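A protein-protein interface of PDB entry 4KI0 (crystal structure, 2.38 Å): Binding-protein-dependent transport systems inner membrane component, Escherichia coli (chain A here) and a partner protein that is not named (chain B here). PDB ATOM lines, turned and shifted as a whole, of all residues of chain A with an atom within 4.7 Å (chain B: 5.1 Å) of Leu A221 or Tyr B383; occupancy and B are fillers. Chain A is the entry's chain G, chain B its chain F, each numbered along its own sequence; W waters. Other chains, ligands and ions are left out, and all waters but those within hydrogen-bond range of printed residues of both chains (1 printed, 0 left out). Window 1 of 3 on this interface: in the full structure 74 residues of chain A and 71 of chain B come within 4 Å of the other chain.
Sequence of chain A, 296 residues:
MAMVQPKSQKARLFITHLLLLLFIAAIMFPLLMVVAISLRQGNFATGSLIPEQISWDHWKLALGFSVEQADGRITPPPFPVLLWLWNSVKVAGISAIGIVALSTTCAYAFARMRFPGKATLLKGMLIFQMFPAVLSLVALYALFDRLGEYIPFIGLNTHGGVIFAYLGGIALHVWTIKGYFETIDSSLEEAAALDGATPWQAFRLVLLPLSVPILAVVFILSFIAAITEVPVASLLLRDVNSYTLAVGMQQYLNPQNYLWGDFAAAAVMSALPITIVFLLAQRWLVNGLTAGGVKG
Val A217 touches Ile B386. Val A217 touches Leu B387. Ile B386 touches Ile A220. Leu A221 touches Tyr B325 (CD2 to CE2, 3.97 Å). Tyr B383 touches Leu A221. Leu A221 touches Leu B387 (CD1 to CD2, 3.7 Å). Ile A224 touches Tyr B325 (CD1 to CD2, 3.7 Å).
Of chain B, only Tyr B325, Tyr B383 and Leu B387 come within 4 Å of Leu A221. Of the printed residues of chain A, Tyr B383 touches Leu A221. Printed residues of chain B within 4 Å of Val A217: Ile B386 and Leu B387. Of the printed residues of chain A, Leu B387 touches Val A217 (3.997 Å) and Leu A221 (3.7 Å). Of the printed residues of chain A, Tyr B325 touches Leu A221 (3.97 Å) and Ile A224 (3.7 Å). Of the printed residues of chain B, Ile A224 touches Tyr B325. Of the printed residues of chain B, Ile A220 touches Ile B386 (3.9 Å). Phe A219 touches none of the printed residues of chain B. The nearest printed residue of chain A that does not touch Tyr B383 is His A173 (6.1 Å).
Of the 10 printed residues of chain A, 4 touch a printed residue of chain B. Hydrophobic or aromatic side chains of chain A within 4 Å of the printed part of chain B: Val A217, Ile A220, Leu A221 and Ile A224. Of the 10 printed residues of chain B, 4 touch a printed residue of chain A. Hydrophobic or aromatic side chains of chain B that line the printed part of chain A: Tyr B325, Tyr B383, Ile B386 and Leu B387. Among the printed residues, 7 pairs touch across the chains. Among the printed residues, no Asp or Glu carboxylate lies within 4 Å of a Lys or Arg side-chain nitrogen of the other chain.
Water W1 lies within hydrogen-bond range of OH of Tyr B325 (2.5 Å) and O of Leu A221 (2.9 Å).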
ATOM      1  N   HIS A 173       7.293  -5.271   1.754  1.00  0.00           N
ATOM      2  CA  HIS A 173       7.408  -5.798   3.104  1.00  0.00           C
ATOM      3  C   HIS A 173       8.325  -4.951   3.981  1.00  0.00           C
ATOM      4  O   HIS A 173       8.062  -4.793   5.177  1.00  0.00           O
ATOM      5  CB  HIS A 173       7.871  -7.251   3.071  1.00  0.00           C
ATOM      6  CG  HIS A 173       6.922  -8.162   2.360  1.00  0.00           C
ATOM      7  ND1 HIS A 173       5.555  -8.085   2.526  1.00  0.00           N
ATOM      8  CD2 HIS A 173       7.137  -9.164   1.476  1.00  0.00           C
ATOM      9  CE1 HIS A 173       4.971  -9.000   1.775  1.00  0.00           C
ATOM     10  NE2 HIS A 173       5.908  -9.669   1.127  1.00  0.00           N
ATOM     11  N   VAL A 217       1.892 -11.005   9.563  1.00  0.00           N
ATOM     12  CA  VAL A 217       1.345 -10.481   8.324  1.00  0.00           C
ATOM     13  C   VAL A 217       2.302 -10.744   7.168  1.00  0.00           C
ATOM     14  O   VAL A 217       1.882 -11.203   6.112  1.00  0.00           O
ATOM     15  CB  VAL A 217       1.044  -8.970   8.427  1.00  0.00           C
ATOM     16  CG1 VAL A 217       0.819  -8.346   7.047  1.00  0.00           C
ATOM     17  CG2 VAL A 217      -0.166  -8.748   9.306  1.00  0.00           C
ATOM     18  N   VAL A 218       3.591 -10.481   7.367  1.00  0.00           N
ATOM     19  CA  VAL A 218       4.558 -10.659   6.279  1.00  0.00           C
ATOM     20  C   VAL A 218       4.763 -12.147   5.958  1.00  0.00           C
ATOM     21  O   VAL A 218       4.898 -12.511   4.795  1.00  0.00           O
ATOM     22  CB  VAL A 218       5.873  -9.900   6.554  1.00  0.00           C
ATOM     23  CG1 VAL A 218       6.925 -10.203   5.501  1.00  0.00           C
ATOM     24  CG2 VAL A 218       5.606  -8.396   6.566  1.00  0.00           C
ATOM     25  N   PHE A 219       4.718 -13.014   6.964  1.00  0.00           N
ATOM     26  CA  PHE A 219       4.852 -14.453   6.713  1.00  0.00           C
ATOM     27  C   PHE A 219       3.648 -14.936   5.913  1.00  0.00           C
ATOM     28  O   PHE A 219       3.792 -15.667   4.935  1.00  0.00           O
ATOM     29  CB  PHE A 219       4.966 -15.238   8.018  1.00  0.00           C
ATOM     30  CG  PHE A 219       5.312 -16.691   7.825  1.00  0.00           C
ATOM     31  CD1 PHE A 219       6.604 -17.144   8.022  1.00  0.00           C
ATOM     32  CD2 PHE A 219       4.349 -17.606   7.445  1.00  0.00           C
ATOM     33  CE1 PHE A 219       6.927 -18.476   7.847  1.00  0.00           C
ATOM     34  CE2 PHE A 219       4.668 -18.942   7.262  1.00  0.00           C
ATOM     35  CZ  PHE A 219       5.957 -19.380   7.467  1.00  0.00           C
ATOM     36  N   ILE A 220       2.466 -14.500   6.331  1.00  0.00           N
ATOM     37  CA  ILE A 220       1.212 -14.888   5.690  1.00  0.00           C
ATOM     38  C   ILE A 220       1.204 -14.469   4.223  1.00  0.00           C
ATOM     39  O   ILE A 220       1.072 -15.306   3.340  1.00  0.00           O
ATOM     40  CB  ILE A 220       0.007 -14.279   6.433  1.00  0.00           C
ATOM     41  CG1 ILE A 220      -0.206 -15.032   7.753  1.00  0.00           C
ATOM     42  CG2 ILE A 220      -1.256 -14.323   5.576  1.00  0.00           C
ATOM     43  CD1 ILE A 220      -1.040 -14.280   8.770  1.00  0.00           C
ATOM     44  N   LEU A 221       1.372 -13.177   3.979  1.00  0.00           N
ATOM     45  CA  LEU A 221       1.403 -12.648   2.618  1.00  0.00           C
ATOM     46  C   LEU A 221       2.435 -13.322   1.709  1.00  0.00           C
ATOM     47  O   LEU A 221       2.171 -13.532   0.528  1.00  0.00           O
ATOM     48  CB  LEU A 221       1.632 -11.138   2.648  1.00  0.00           C
ATOM     49  CG  LEU A 221       0.427 -10.337   3.156  1.00  0.00           C
ATOM     50  CD1 LEU A 221       0.716  -8.844   3.104  1.00  0.00           C
ATOM     51  CD2 LEU A 221      -0.834 -10.654   2.360  1.00  0.00           C
ATOM     52  N   SER A 222       3.588 -13.685   2.267  1.00  0.00           N
ATOM     53  CA  SER A 222       4.673 -14.316   1.501  1.00  0.00           C
ATOM     54  C   SER A 222       4.417 -15.782   1.192  1.00  0.00           C
ATOM     55  O   SER A 222       4.813 -16.294   0.140  1.00  0.00           O
ATOM     56  CB  SER A 222       5.980 -14.211   2.277  1.00  0.00           C
ATOM     57  OG  SER A 222       6.289 -12.856   2.510  1.00  0.00           O
ATOM     58  N   PHE A 223       3.793 -16.470   2.135  1.00  0.00           N
ATOM     59  CA  PHE A 223       3.440 -17.871   1.952  1.00  0.00           C
ATOM     60  C   PHE A 223       2.430 -17.963   0.802  1.00  0.00           C
ATOM     61  O   PHE A 223       2.674 -18.632  -0.191  1.00  0.00           O
ATOM     62  CB  PHE A 223       2.876 -18.427   3.255  1.00  0.00           C
ATOM     63  CG  PHE A 223       2.768 -19.914   3.288  1.00  0.00           C
ATOM     64  CD1 PHE A 223       3.880 -20.694   3.573  1.00  0.00           C
ATOM     65  CD2 PHE A 223       1.555 -20.537   3.066  1.00  0.00           C
ATOM     66  CE1 PHE A 223       3.784 -22.073   3.632  1.00  0.00           C
ATOM     67  CE2 PHE A 223       1.450 -21.919   3.124  1.00  0.00           C
ATOM     68  CZ  PHE A 223       2.567 -22.689   3.404  1.00  0.00           C
ATOM     69  N   ILE A 224       1.333 -17.226   0.927  1.00  0.00           N
ATOM     70  CA  ILE A 224       0.299 -17.134  -0.104  1.00  0.00           C
ATOM     71  C   ILE A 224       0.910 -16.862  -1.477  1.00  0.00           C
ATOM     72  O   ILE A 224       0.741 -17.644  -2.409  1.00  0.00           O
ATOM     73  CB  ILE A 224      -0.724 -16.032   0.245  1.00  0.00           C
ATOM     74  CG1 ILE A 224      -1.559 -16.458   1.455  1.00  0.00           C
ATOM     75  CG2 ILE A 224      -1.655 -15.766  -0.926  1.00  0.00           C
ATOM     76  CD1 ILE A 224      -2.476 -15.381   1.991  1.00  0.00           C
ATOM     77  N   ALA A 225       1.652 -15.770  -1.589  1.00  0.00           N
ATOM     78  CA  ALA A 225       2.324 -15.454  -2.832  1.00  0.00           C
ATOM     79  C   ALA A 225       3.033 -16.691  -3.414  1.00  0.00           C
ATOM     80  O   ALA A 225       2.778 -17.074  -4.558  1.00  0.00           O
ATOM     81  CB  ALA A 225       3.296 -14.310  -2.622  1.00  0.00           C
ATOM     82  N   TYR B 325      -8.551 -15.614  -1.239  1.00  0.00           N
ATOM     83  CA  TYR B 325      -7.137 -15.402  -1.497  1.00  0.00           C
ATOM     84  C   TYR B 325      -6.352 -16.702  -1.364  1.00  0.00           C
ATOM     85  O   TYR B 325      -5.227 -16.796  -1.851  1.00  0.00           O
ATOM     86  CB  TYR B 325      -6.639 -14.350  -0.509  1.00  0.00           C
ATOM     87  CG  TYR B 325      -5.361 -13.617  -0.843  1.00  0.00           C
ATOM     88  CD1 TYR B 325      -4.893 -13.493  -2.154  1.00  0.00           C
ATOM     89  CD2 TYR B 325      -4.639 -13.002   0.170  1.00  0.00           C
ATOM     90  CE1 TYR B 325      -3.725 -12.795  -2.428  1.00  0.00           C
ATOM     91  CE2 TYR B 325      -3.481 -12.306  -0.097  1.00  0.00           C
ATOM     92  CZ  TYR B 325      -3.031 -12.201  -1.391  1.00  0.00           C
ATOM     93  OH  TYR B 325      -1.874 -11.506  -1.619  1.00  0.00           O
ATOM     94  N   GLY B 380      -9.229  -8.810  -4.135  1.00  0.00           N
ATOM     95  CA  GLY B 380      -8.250  -7.936  -3.477  1.00  0.00           C
ATOM     96  C   GLY B 380      -8.464  -7.592  -2.014  1.00  0.00           C
ATOM     97  O   GLY B 380      -7.518  -7.185  -1.332  1.00  0.00           O
ATOM     98  N   TYR B 381      -9.684  -7.748  -1.507  1.00  0.00           N
ATOM     99  CA  TYR B 381      -9.948  -7.342  -0.125  1.00  0.00           C
ATOM    100  C   TYR B 381      -9.149  -8.152   0.903  1.00  0.00           C
ATOM    101  O   TYR B 381      -8.706  -7.592   1.900  1.00  0.00           O
ATOM    102  CB  TYR B 381     -11.455  -7.321   0.201  1.00  0.00           C
ATOM    103  CG  TYR B 381     -12.058  -8.642   0.634  1.00  0.00           C
ATOM    104  CD1 TYR B 381     -11.867  -9.130   1.923  1.00  0.00           C
ATOM    105  CD2 TYR B 381     -12.849  -9.381  -0.232  1.00  0.00           C
ATOM    106  CE1 TYR B 381     -12.429 -10.332   2.325  1.00  0.00           C
ATOM    107  CE2 TYR B 381     -13.410 -10.583   0.158  1.00  0.00           C
ATOM    108  CZ  TYR B 381     -13.197 -11.057   1.436  1.00  0.00           C
ATOM    109  OH  TYR B 381     -13.745 -12.262   1.818  1.00  0.00           O
ATOM    110  N   PRO B 382      -8.946  -9.464   0.670  1.00  0.00           N
ATOM    111  CA  PRO B 382      -8.210 -10.239   1.685  1.00  0.00           C
ATOM    112  C   PRO B 382      -6.800  -9.729   1.963  1.00  0.00           C
ATOM    113  O   PRO B 382      -6.335  -9.761   3.107  1.00  0.00           O
ATOM    114  CB  PRO B 382      -8.166 -11.638   1.080  1.00  0.00           C
ATOM    115  CG  PRO B 382      -9.387 -11.697   0.211  1.00  0.00           C
ATOM    116  CD  PRO B 382      -9.424 -10.337  -0.419  1.00  0.00           C
ATOM    117  N   TYR B 383      -6.136  -9.257   0.920  1.00  0.00           N
ATOM    118  CA  TYR B 383      -4.814  -8.656   1.036  1.00  0.00           C
ATOM    119  C   TYR B 383      -4.847  -7.483   1.989  1.00  0.00           C
ATOM    120  O   TYR B 383      -4.042  -7.392   2.910  1.00  0.00           O
ATOM    121  CB  TYR B 383      -4.361  -8.177  -0.338  1.00  0.00           C
ATOM    122  CG  TYR B 383      -3.055  -7.438  -0.362  1.00  0.00           C
ATOM    123  CD1 TYR B 383      -1.869  -8.068  -0.009  1.00  0.00           C
ATOM    124  CD2 TYR B 383      -2.993  -6.112  -0.782  1.00  0.00           C
ATOM    125  CE1 TYR B 383      -0.662  -7.399  -0.053  1.00  0.00           C
ATOM    126  CE2 TYR B 383      -1.783  -5.439  -0.828  1.00  0.00           C
ATOM    127  CZ  TYR B 383      -0.622  -6.095  -0.463  1.00  0.00           C
ATOM    128  OH  TYR B 383       0.580  -5.432  -0.495  1.00  0.00           O
ATOM    129  N   MET B 384      -5.802  -6.590   1.762  1.00  0.00           N
ATOM    130  CA  MET B 384      -5.898  -5.374   2.548  1.00  0.00           C
ATOM    131  C   MET B 384      -6.345  -5.670   3.970  1.00  0.00           C
ATOM    132  O   MET B 384      -5.897  -5.025   4.906  1.00  0.00           O
ATOM    133  CB  MET B 384      -6.825  -4.367   1.857  1.00  0.00           C
ATOM    134  CG  MET B 384      -6.140  -3.648   0.704  1.00  0.00           C
ATOM    135  SD  MET B 384      -4.683  -2.770   1.295  1.00  0.00           S
ATOM    136  CE  MET B 384      -3.838  -2.330  -0.218  1.00  0.00           C
ATOM    137  N   MET B 385      -7.213  -6.663   4.111  1.00  0.00           N
ATOM    138  CA  MET B 385      -7.671  -7.144   5.397  1.00  0.00           C
ATOM    139  C   MET B 385      -6.507  -7.675   6.229  1.00  0.00           C
ATOM    140  O   MET B 385      -6.349  -7.313   7.387  1.00  0.00           O
ATOM    141  CB  MET B 385      -8.710  -8.256   5.193  1.00  0.00           C
ATOM    142  CG  MET B 385      -9.422  -8.681   6.471  1.00  0.00           C
ATOM    143  SD  MET B 385     -10.419 -10.157   6.232  1.00  0.00           S
ATOM    144  CE  MET B 385     -10.865 -10.537   7.924  1.00  0.00           C
ATOM    145  N   ILE B 386      -5.683  -8.526   5.635  1.00  0.00           N
ATOM    146  CA  ILE B 386      -4.581  -9.141   6.374  1.00  0.00           C
ATOM    147  C   ILE B 386      -3.573  -8.082   6.829  1.00  0.00           C
ATOM    148  O   ILE B 386      -3.119  -8.097   7.977  1.00  0.00           O
ATOM    149  CB  ILE B 386      -3.908 -10.253   5.546  1.00  0.00           C
ATOM    150  CG1 ILE B 386      -4.877 -11.432   5.397  1.00  0.00           C
ATOM    151  CG2 ILE B 386      -2.635 -10.733   6.228  1.00  0.00           C
ATOM    152  CD1 ILE B 386      -4.525 -12.395   4.286  1.00  0.00           C
ATOM    153  N   LEU B 387      -3.231  -7.160   5.933  1.00  0.00           N
ATOM    154  CA  LEU B 387      -2.433  -6.000   6.324  1.00  0.00           C
ATOM    155  C   LEU B 387      -3.062  -5.296   7.529  1.00  0.00           C
ATOM    156  O   LEU B 387      -2.416  -5.131   8.553  1.00  0.00           O
ATOM    157  CB  LEU B 387      -2.320  -5.010   5.167  1.00  0.00           C
ATOM    158  CG  LEU B 387      -1.440  -5.436   3.999  1.00  0.00           C
ATOM    159  CD1 LEU B 387      -1.702  -4.502   2.829  1.00  0.00           C
ATOM    160  CD2 LEU B 387       0.027  -5.463   4.395  1.00  0.00           C
ATOM    161  N   LEU B 429       1.424   1.135   0.632  1.00  0.00           N
ATOM    162  CA  LEU B 429       0.757  -0.081   0.170  1.00  0.00           C
ATOM    163  C   LEU B 429      -0.356   0.205  -0.833  1.00  0.00           C
ATOM    164  O   LEU B 429      -0.561  -0.570  -1.760  1.00  0.00           O
ATOM    165  CB  LEU B 429       0.190  -0.862   1.350  1.00  0.00           C
ATOM    166  CG  LEU B 429       1.229  -1.359   2.356  1.00  0.00           C
ATOM    167  CD1 LEU B 429       0.534  -1.722   3.658  1.00  0.00           C
ATOM    168  CD2 LEU B 429       2.030  -2.533   1.817  1.00  0.00           C
HETATM  169  O   HOH W   1       0.583 -11.650  -1.031  1.00  0.00           O
